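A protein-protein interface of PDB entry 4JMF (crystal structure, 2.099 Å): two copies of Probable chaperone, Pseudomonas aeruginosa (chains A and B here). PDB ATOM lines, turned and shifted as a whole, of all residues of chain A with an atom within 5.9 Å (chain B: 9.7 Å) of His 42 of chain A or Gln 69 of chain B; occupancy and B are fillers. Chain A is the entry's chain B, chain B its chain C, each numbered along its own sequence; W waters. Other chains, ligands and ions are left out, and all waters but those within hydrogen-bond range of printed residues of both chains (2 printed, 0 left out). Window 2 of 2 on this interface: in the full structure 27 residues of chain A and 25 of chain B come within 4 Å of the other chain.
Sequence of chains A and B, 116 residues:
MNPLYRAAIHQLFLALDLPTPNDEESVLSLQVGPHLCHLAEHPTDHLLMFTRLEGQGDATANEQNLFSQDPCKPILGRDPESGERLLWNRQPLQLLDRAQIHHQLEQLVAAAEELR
Water W2 lies within hydrogen-bond range of NH2 of Arg 90 of chain A (2.6 Å) and O of Pro 71 of chain B (3.4 Å). Water W1 lies within hydrogen-bond range of NH2 of Arg 90 of chain A (2.6 Å), O of Asp 70 of chain B (2.9 Å) and N of Ser 68 of chain B (2.9 Å).
Among the printed residues, merely in contact across the chains: His 42 of chain A with Phe 67 of chain B, His 42 of chain A with Ser 68 of chain B, His 42 of chain A with Gln 69 of chain B, Pro 43 of chain A with Gln 69 of chain B, Pro 43 of chain A with Pro 71 of chain B, His 46 of chain A with Pro 71 of chain B, Leu 48 of chain A with Phe 67 of chain B and Arg 90 of chain A with Pro 71 of chain B.
The backbone carbonyl oxygen (O) of Ala 40 of chain A lies within hydrogen-bond range of the backbone NH (N) of Leu 48 of chain A (2.8 Å). The guanidinium group (NH1) of Arg 90 of chain A sits close to the backbone carbonyl oxygen (O) of His 42 of chain A. O of Thr 44 of chain A sits at hydrogen-bond distance from ND1 of His 46 of chain A, 3.1 Å away. OG of Ser 68 of chain B lies within hydrogen-bond range of N of Asp 70 of chain B, 3.1 Å away.
The backbone carbonyl oxygen (O) of Ser 68 of chain B is in hydrogen-bond range of the guanidinium group (NH1) of Arg 90 of chain A.
Of chain B, only Phe 67, Ser 68 and Gln 69 come within 4 Å of His 42 of chain A. Gln 69 of chain B touches just these residues of chain A: His 42 (3.9 Å) and Pro 43 (3.3 Å). Of chain B, only Gln 69 (3.3 Å) and Pro 71 (3.9 Å) come within 4 Å of Pro 43 of chain A. Printed residues of chain A within 4 Å of Phe 67 of chain B: His 42 and Leu 48. Of the printed residues of chain B, Leu 48 of chain A touches Phe 67. The nearest residue of chain B that does not touch His 42 of chain A is Asp 70 of chain B (6.1 Å). The nearest printed residue of chain B that does not touch Leu 48 of chain A is Ser 68 of chain B (6.6 Å).
No position is printed for both chains.
Hydrophobic or aromatic side chains of chain A that line the printed part of chain B: His 42, Pro 43, His 46 and Leu 48. Hydrophobic or aromatic side chains of chain B within 4 Å of the printed part of chain A: Phe 67 and Pro 71. Among the printed residues, 9 pairs touch across the chains.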
ATOM      1  N   ALA A  40     -16.388  18.907  26.584  1.00  0.00           N
ATOM      2  CA  ALA A  40     -17.120  19.304  27.771  1.00  0.00           C
ATOM      3  C   ALA A  40     -18.577  19.434  27.423  1.00  0.00           C
ATOM      4  O   ALA A  40     -18.917  19.684  26.271  1.00  0.00           O
ATOM      5  CB  ALA A  40     -16.589  20.643  28.294  1.00  0.00           C
ATOM      6  N   GLU A  41     -19.441  19.276  28.414  1.00  0.00           N
ATOM      7  CA  GLU A  41     -20.840  19.601  28.210  1.00  0.00           C
ATOM      8  C   GLU A  41     -21.016  21.114  28.356  1.00  0.00           C
ATOM      9  O   GLU A  41     -20.844  21.660  29.444  1.00  0.00           O
ATOM     10  CB  GLU A  41     -21.725  18.897  29.230  1.00  0.00           C
ATOM     11  CG  GLU A  41     -23.197  19.126  28.933  1.00  0.00           C
ATOM     12  CD  GLU A  41     -24.125  18.457  29.929  1.00  0.00           C
ATOM     13  OE1 GLU A  41     -23.659  18.015  31.008  1.00  0.00           O
ATOM     14  OE2 GLU A  41     -25.337  18.385  29.628  1.00  0.00           O
ATOM     15  N   HIS A  42     -21.373  21.795  27.271  1.00  0.00           N
ATOM     16  CA  HIS A  42     -21.402  23.257  27.313  1.00  0.00           C
ATOM     17  C   HIS A  42     -22.153  23.809  26.123  1.00  0.00           C
ATOM     18  O   HIS A  42     -21.696  23.669  24.992  1.00  0.00           O
ATOM     19  CB  HIS A  42     -19.974  23.809  27.311  1.00  0.00           C
ATOM     20  CG  HIS A  42     -19.890  25.275  27.605  1.00  0.00           C
ATOM     21  ND1 HIS A  42     -19.939  26.237  26.618  1.00  0.00           N
ATOM     22  CD2 HIS A  42     -19.749  25.945  28.775  1.00  0.00           C
ATOM     23  CE1 HIS A  42     -19.827  27.438  27.164  1.00  0.00           C
ATOM     24  NE2 HIS A  42     -19.711  27.288  28.472  1.00  0.00           N
ATOM     25  N   PRO A  43     -23.337  24.396  26.359  1.00  0.00           N
ATOM     26  CA  PRO A  43     -24.045  24.423  27.644  1.00  0.00           C
ATOM     27  C   PRO A  43     -24.660  23.066  27.870  1.00  0.00           C
ATOM     28  O   PRO A  43     -24.329  22.118  27.140  1.00  0.00           O
ATOM     29  CB  PRO A  43     -25.165  25.444  27.408  1.00  0.00           C
ATOM     30  CG  PRO A  43     -25.441  25.336  25.914  1.00  0.00           C
ATOM     31  CD  PRO A  43     -24.104  25.042  25.279  1.00  0.00           C
ATOM     32  N   THR A  44     -25.531  22.970  28.867  1.00  0.00           N
ATOM     33  CA  THR A  44     -26.251  21.740  29.146  1.00  0.00           C
ATOM     34  C   THR A  44     -26.834  21.148  27.862  1.00  0.00           C
ATOM     35  O   THR A  44     -27.339  21.882  26.999  1.00  0.00           O
ATOM     36  CB  THR A  44     -27.345  22.012  30.180  1.00  0.00           C
ATOM     37  OG1 THR A  44     -26.717  22.554  31.342  1.00  0.00           O
ATOM     38  CG2 THR A  44     -28.068  20.722  30.580  1.00  0.00           C
ATOM     39  N   ASP A  45     -26.697  19.829  27.725  1.00  0.00           N
ATOM     40  CA  ASP A  45     -27.213  19.069  26.576  1.00  0.00           C
ATOM     41  C   ASP A  45     -26.517  19.332  25.246  1.00  0.00           C
ATOM     42  O   ASP A  45     -26.999  18.886  24.201  1.00  0.00           O
ATOM     43  CB  ASP A  45     -28.733  19.239  26.432  1.00  0.00           C
ATOM     44  CG  ASP A  45     -29.493  18.653  27.605  1.00  0.00           C
ATOM     45  OD1 ASP A  45     -29.153  17.526  28.034  1.00  0.00           O
ATOM     46  OD2 ASP A  45     -30.412  19.329  28.108  1.00  0.00           O
ATOM     47  N   HIS A  46     -25.383  20.030  25.279  1.00  0.00           N
ATOM     48  CA  HIS A  46     -24.533  20.140  24.085  1.00  0.00           C
ATOM     49  C   HIS A  46     -23.120  19.659  24.373  1.00  0.00           C
ATOM     50  O   HIS A  46     -22.645  19.742  25.505  1.00  0.00           O
ATOM     51  CB  HIS A  46     -24.473  21.578  23.558  1.00  0.00           C
ATOM     52  CG  HIS A  46     -25.790  22.116  23.103  1.00  0.00           C
ATOM     53  ND1 HIS A  46     -26.823  22.383  23.976  1.00  0.00           N
ATOM     54  CD2 HIS A  46     -26.237  22.459  21.871  1.00  0.00           C
ATOM     55  CE1 HIS A  46     -27.849  22.867  23.302  1.00  0.00           C
ATOM     56  NE2 HIS A  46     -27.526  22.911  22.023  1.00  0.00           N
ATOM     57  N   LEU A  47     -22.448  19.142  23.350  1.00  0.00           N
ATOM     58  CA  LEU A  47     -21.072  18.679  23.509  1.00  0.00           C
ATOM     59  C   LEU A  47     -20.150  19.644  22.784  1.00  0.00           C
ATOM     60  O   LEU A  47     -20.244  19.804  21.561  1.00  0.00           O
ATOM     61  CB  LEU A  47     -20.895  17.276  22.918  1.00  0.00           C
ATOM     62  CG  LEU A  47     -19.453  16.776  22.769  1.00  0.00           C
ATOM     63  CD1 LEU A  47     -18.762  16.691  24.120  1.00  0.00           C
ATOM     64  CD2 LEU A  47     -19.448  15.413  22.137  1.00  0.00           C
ATOM     65  N   LEU A  48     -19.264  20.279  23.542  1.00  0.00           N
ATOM     66  CA  LEU A  48     -18.307  21.219  22.975  1.00  0.00           C
ATOM     67  C   LEU A  48     -16.966  20.519  22.834  1.00  0.00           C
ATOM     68  O   LEU A  48     -16.476  19.945  23.799  1.00  0.00           O
ATOM     69  CB  LEU A  48     -18.163  22.424  23.903  1.00  0.00           C
ATOM     70  CG  LEU A  48     -17.166  23.519  23.530  1.00  0.00           C
ATOM     71  CD1 LEU A  48     -17.690  24.357  22.349  1.00  0.00           C
ATOM     72  CD2 LEU A  48     -16.874  24.402  24.755  1.00  0.00           C
ATOM     73  N   ARG A  90     -19.499  22.351  18.162  1.00  0.00           N
ATOM     74  CA  ARG A  90     -20.477  21.957  19.175  1.00  0.00           C
ATOM     75  C   ARG A  90     -21.658  21.239  18.548  1.00  0.00           C
ATOM     76  O   ARG A  90     -22.105  21.605  17.455  1.00  0.00           O
ATOM     77  CB  ARG A  90     -20.978  23.179  19.947  1.00  0.00           C
ATOM     78  CG  ARG A  90     -22.076  22.840  20.951  1.00  0.00           C
ATOM     79  CD  ARG A  90     -22.104  23.838  22.083  1.00  0.00           C
ATOM     80  NE  ARG A  90     -22.281  25.155  21.556  1.00  0.00           N
ATOM     81  CZ  ARG A  90     -21.876  26.281  22.129  1.00  0.00           C
ATOM     82  NH1 ARG A  90     -21.253  26.306  23.317  1.00  0.00           N
ATOM     83  NH2 ARG A  90     -22.117  27.394  21.476  1.00  0.00           N
ATOM     84  N   LEU B  66     -15.671  33.381  19.485  1.00  0.00           N
ATOM     85  CA  LEU B  66     -15.483  32.429  20.570  1.00  0.00           C
ATOM     86  C   LEU B  66     -16.859  31.975  21.028  1.00  0.00           C
ATOM     87  O   LEU B  66     -17.802  32.775  21.079  1.00  0.00           O
ATOM     88  CB  LEU B  66     -14.736  33.054  21.758  1.00  0.00           C
ATOM     89  CG  LEU B  66     -14.492  32.094  22.940  1.00  0.00           C
ATOM     90  CD1 LEU B  66     -13.469  31.043  22.554  1.00  0.00           C
ATOM     91  CD2 LEU B  66     -14.068  32.803  24.234  1.00  0.00           C
ATOM     92  N   PHE B  67     -16.982  30.702  21.379  1.00  0.00           N
ATOM     93  CA  PHE B  67     -18.254  30.191  21.885  1.00  0.00           C
ATOM     94  C   PHE B  67     -18.652  30.890  23.173  1.00  0.00           C
ATOM     95  O   PHE B  67     -17.787  31.364  23.919  1.00  0.00           O
ATOM     96  CB  PHE B  67     -18.118  28.694  22.166  1.00  0.00           C
ATOM     97  CG  PHE B  67     -16.986  28.360  23.090  1.00  0.00           C
ATOM     98  CD1 PHE B  67     -17.141  28.456  24.476  1.00  0.00           C
ATOM     99  CD2 PHE B  67     -15.767  27.936  22.580  1.00  0.00           C
ATOM    100  CE1 PHE B  67     -16.091  28.144  25.336  1.00  0.00           C
ATOM    101  CE2 PHE B  67     -14.713  27.621  23.424  1.00  0.00           C
ATOM    102  CZ  PHE B  67     -14.874  27.729  24.809  1.00  0.00           C
ATOM    103  N   SER B  68     -19.956  30.933  23.444  1.00  0.00           N
ATOM    104  CA  SER B  68     -20.461  31.368  24.742  1.00  0.00           C
ATOM    105  C   SER B  68     -21.454  30.311  25.210  1.00  0.00           C
ATOM    106  O   SER B  68     -21.522  29.227  24.623  1.00  0.00           O
ATOM    107  CB  SER B  68     -21.146  32.729  24.626  1.00  0.00           C
ATOM    108  OG  SER B  68     -22.418  32.593  24.019  1.00  0.00           O
ATOM    109  N   GLN B  69     -22.224  30.605  26.251  1.00  0.00           N
ATOM    110  CA  GLN B  69     -23.227  29.647  26.730  1.00  0.00           C
ATOM    111  C   GLN B  69     -24.410  29.543  25.785  1.00  0.00           C
ATOM    112  O   GLN B  69     -25.214  28.619  25.892  1.00  0.00           O
ATOM    113  CB  GLN B  69     -23.757  30.043  28.109  1.00  0.00           C
ATOM    114  CG  GLN B  69     -22.685  30.185  29.170  1.00  0.00           C
ATOM    115  CD  GLN B  69     -22.702  29.051  30.166  1.00  0.00           C
ATOM    116  OE1 GLN B  69     -23.384  28.039  29.963  1.00  0.00           O
ATOM    117  NE2 GLN B  69     -21.942  29.204  31.253  1.00  0.00           N
ATOM    118  N   ASP B  70     -24.528  30.507  24.881  1.00  0.00           N
ATOM    119  CA  ASP B  70     -25.650  30.558  23.950  1.00  0.00           C
ATOM    120  C   ASP B  70     -25.268  30.006  22.565  1.00  0.00           C
ATOM    121  O   ASP B  70     -24.553  30.667  21.812  1.00  0.00           O
ATOM    122  CB  ASP B  70     -26.131  32.009  23.816  1.00  0.00           C
ATOM    123  CG  ASP B  70     -27.451  32.123  23.075  1.00  0.00           C
ATOM    124  OD1 ASP B  70     -27.876  31.131  22.439  1.00  0.00           O
ATOM    125  OD2 ASP B  70     -28.066  33.212  23.118  1.00  0.00           O
ATOM    126  N   PRO B  71     -25.769  28.806  22.214  1.00  0.00           N
ATOM    127  CA  PRO B  71     -25.455  28.201  20.906  1.00  0.00           C
ATOM    128  C   PRO B  71     -25.855  29.077  19.725  1.00  0.00           C
ATOM    129  O   PRO B  71     -25.307  28.894  18.627  1.00  0.00           O
ATOM    130  CB  PRO B  71     -26.288  26.912  20.900  1.00  0.00           C
ATOM    131  CG  PRO B  71     -26.459  26.563  22.374  1.00  0.00           C
ATOM    132  CD  PRO B  71     -26.581  27.912  23.067  1.00  0.00           C
ATOM    133  N   CYS B  72     -26.785  30.009  19.942  1.00  0.00           N
ATOM    134  CA  CYS B  72     -27.175  30.956  18.896  1.00  0.00           C
ATOM    135  C   CYS B  72     -26.311  32.219  18.780  1.00  0.00           C
ATOM    136  O   CYS B  72     -26.611  33.094  17.969  1.00  0.00           O
ATOM    137  CB  CYS B  72     -28.627  31.366  19.080  1.00  0.00           C
ATOM    138  SG  CYS B  72     -29.757  30.024  18.782  1.00  0.00           S
ATOM    139  N   LYS B  73     -25.256  32.330  19.582  1.00  0.00           N
ATOM    140  CA  LYS B  73     -24.354  33.476  19.438  1.00  0.00           C
ATOM    141  C   LYS B  73     -23.806  33.484  18.019  1.00  0.00           C
ATOM    142  O   LYS B  73     -23.242  32.483  17.566  1.00  0.00           O
ATOM    143  CB  LYS B  73     -23.199  33.414  20.446  1.00  0.00           C
ATOM    144  CG  LYS B  73     -22.257  34.600  20.326  1.00  0.00           C
ATOM    145  CD  LYS B  73     -21.032  34.472  21.224  1.00  0.00           C
ATOM    146  CE  LYS B  73     -20.089  35.656  20.979  1.00  0.00           C
ATOM    147  NZ  LYS B  73     -18.762  35.504  21.658  1.00  0.00           N
ATOM    148  N   GLN B 100     -37.488  29.771  20.774  1.00  0.00           N
ATOM    149  CA  GLN B 100     -36.111  29.476  20.398  1.00  0.00           C
ATOM    150  C   GLN B 100     -35.799  29.871  18.947  1.00  0.00           C
ATOM    151  O   GLN B 100     -34.652  30.181  18.620  1.00  0.00           O
ATOM    152  CB  GLN B 100     -35.815  27.993  20.655  1.00  0.00           C
ATOM    153  CG  GLN B 100     -34.336  27.614  20.679  1.00  0.00           C
ATOM    154  CD  GLN B 100     -33.473  28.515  21.570  1.00  0.00           C
ATOM    155  OE1 GLN B 100     -33.935  29.048  22.583  1.00  0.00           O
ATOM    156  NE2 GLN B 100     -32.205  28.681  21.185  1.00  0.00           N
ATOM    157  N   HIS B 103     -35.617  33.678  19.109  1.00  0.00           N
ATOM    158  CA  HIS B 103     -34.378  33.976  19.820  1.00  0.00           C
ATOM    159  C   HIS B 103     -33.182  33.981  18.873  1.00  0.00           C
ATOM    160  O   HIS B 103     -32.303  34.847  18.977  1.00  0.00           O
ATOM    161  CB  HIS B 103     -34.162  32.985  20.970  1.00  0.00           C
ATOM    162  CG  HIS B 103     -32.909  33.227  21.758  1.00  0.00           C
ATOM    163  ND1 HIS B 103     -32.810  34.214  22.717  1.00  0.00           N
ATOM    164  CD2 HIS B 103     -31.705  32.603  21.734  1.00  0.00           C
ATOM    165  CE1 HIS B 103     -31.602  34.183  23.254  1.00  0.00           C
ATOM    166  NE2 HIS B 103     -30.913  33.214  22.676  1.00  0.00           N
ATOM    167  N   GLN B 107     -30.729  37.256  18.408  1.00  0.00           N
ATOM    168  CA  GLN B 107     -29.279  37.178  18.513  1.00  0.00           C
ATOM    169  C   GLN B 107     -28.566  37.684  17.275  1.00  0.00           C
ATOM    170  O   GLN B 107     -27.562  38.401  17.378  1.00  0.00           O
ATOM    171  CB  GLN B 107     -28.860  35.737  18.809  1.00  0.00           C
ATOM    172  CG  GLN B 107     -29.145  35.318  20.237  1.00  0.00           C
ATOM    173  CD  GLN B 107     -28.309  36.111  21.220  1.00  0.00           C
ATOM    174  OE1 GLN B 107     -27.088  36.218  21.065  1.00  0.00           O
ATOM    175  NE2 GLN B 107     -28.960  36.690  22.228  1.00  0.00           N
HETATM  176  O   HOH W   1     -21.789  30.015  21.391  1.00  0.00           O
HETATM  177  O   HOH W   2     -22.946  26.470  19.208  1.00  0.00           O
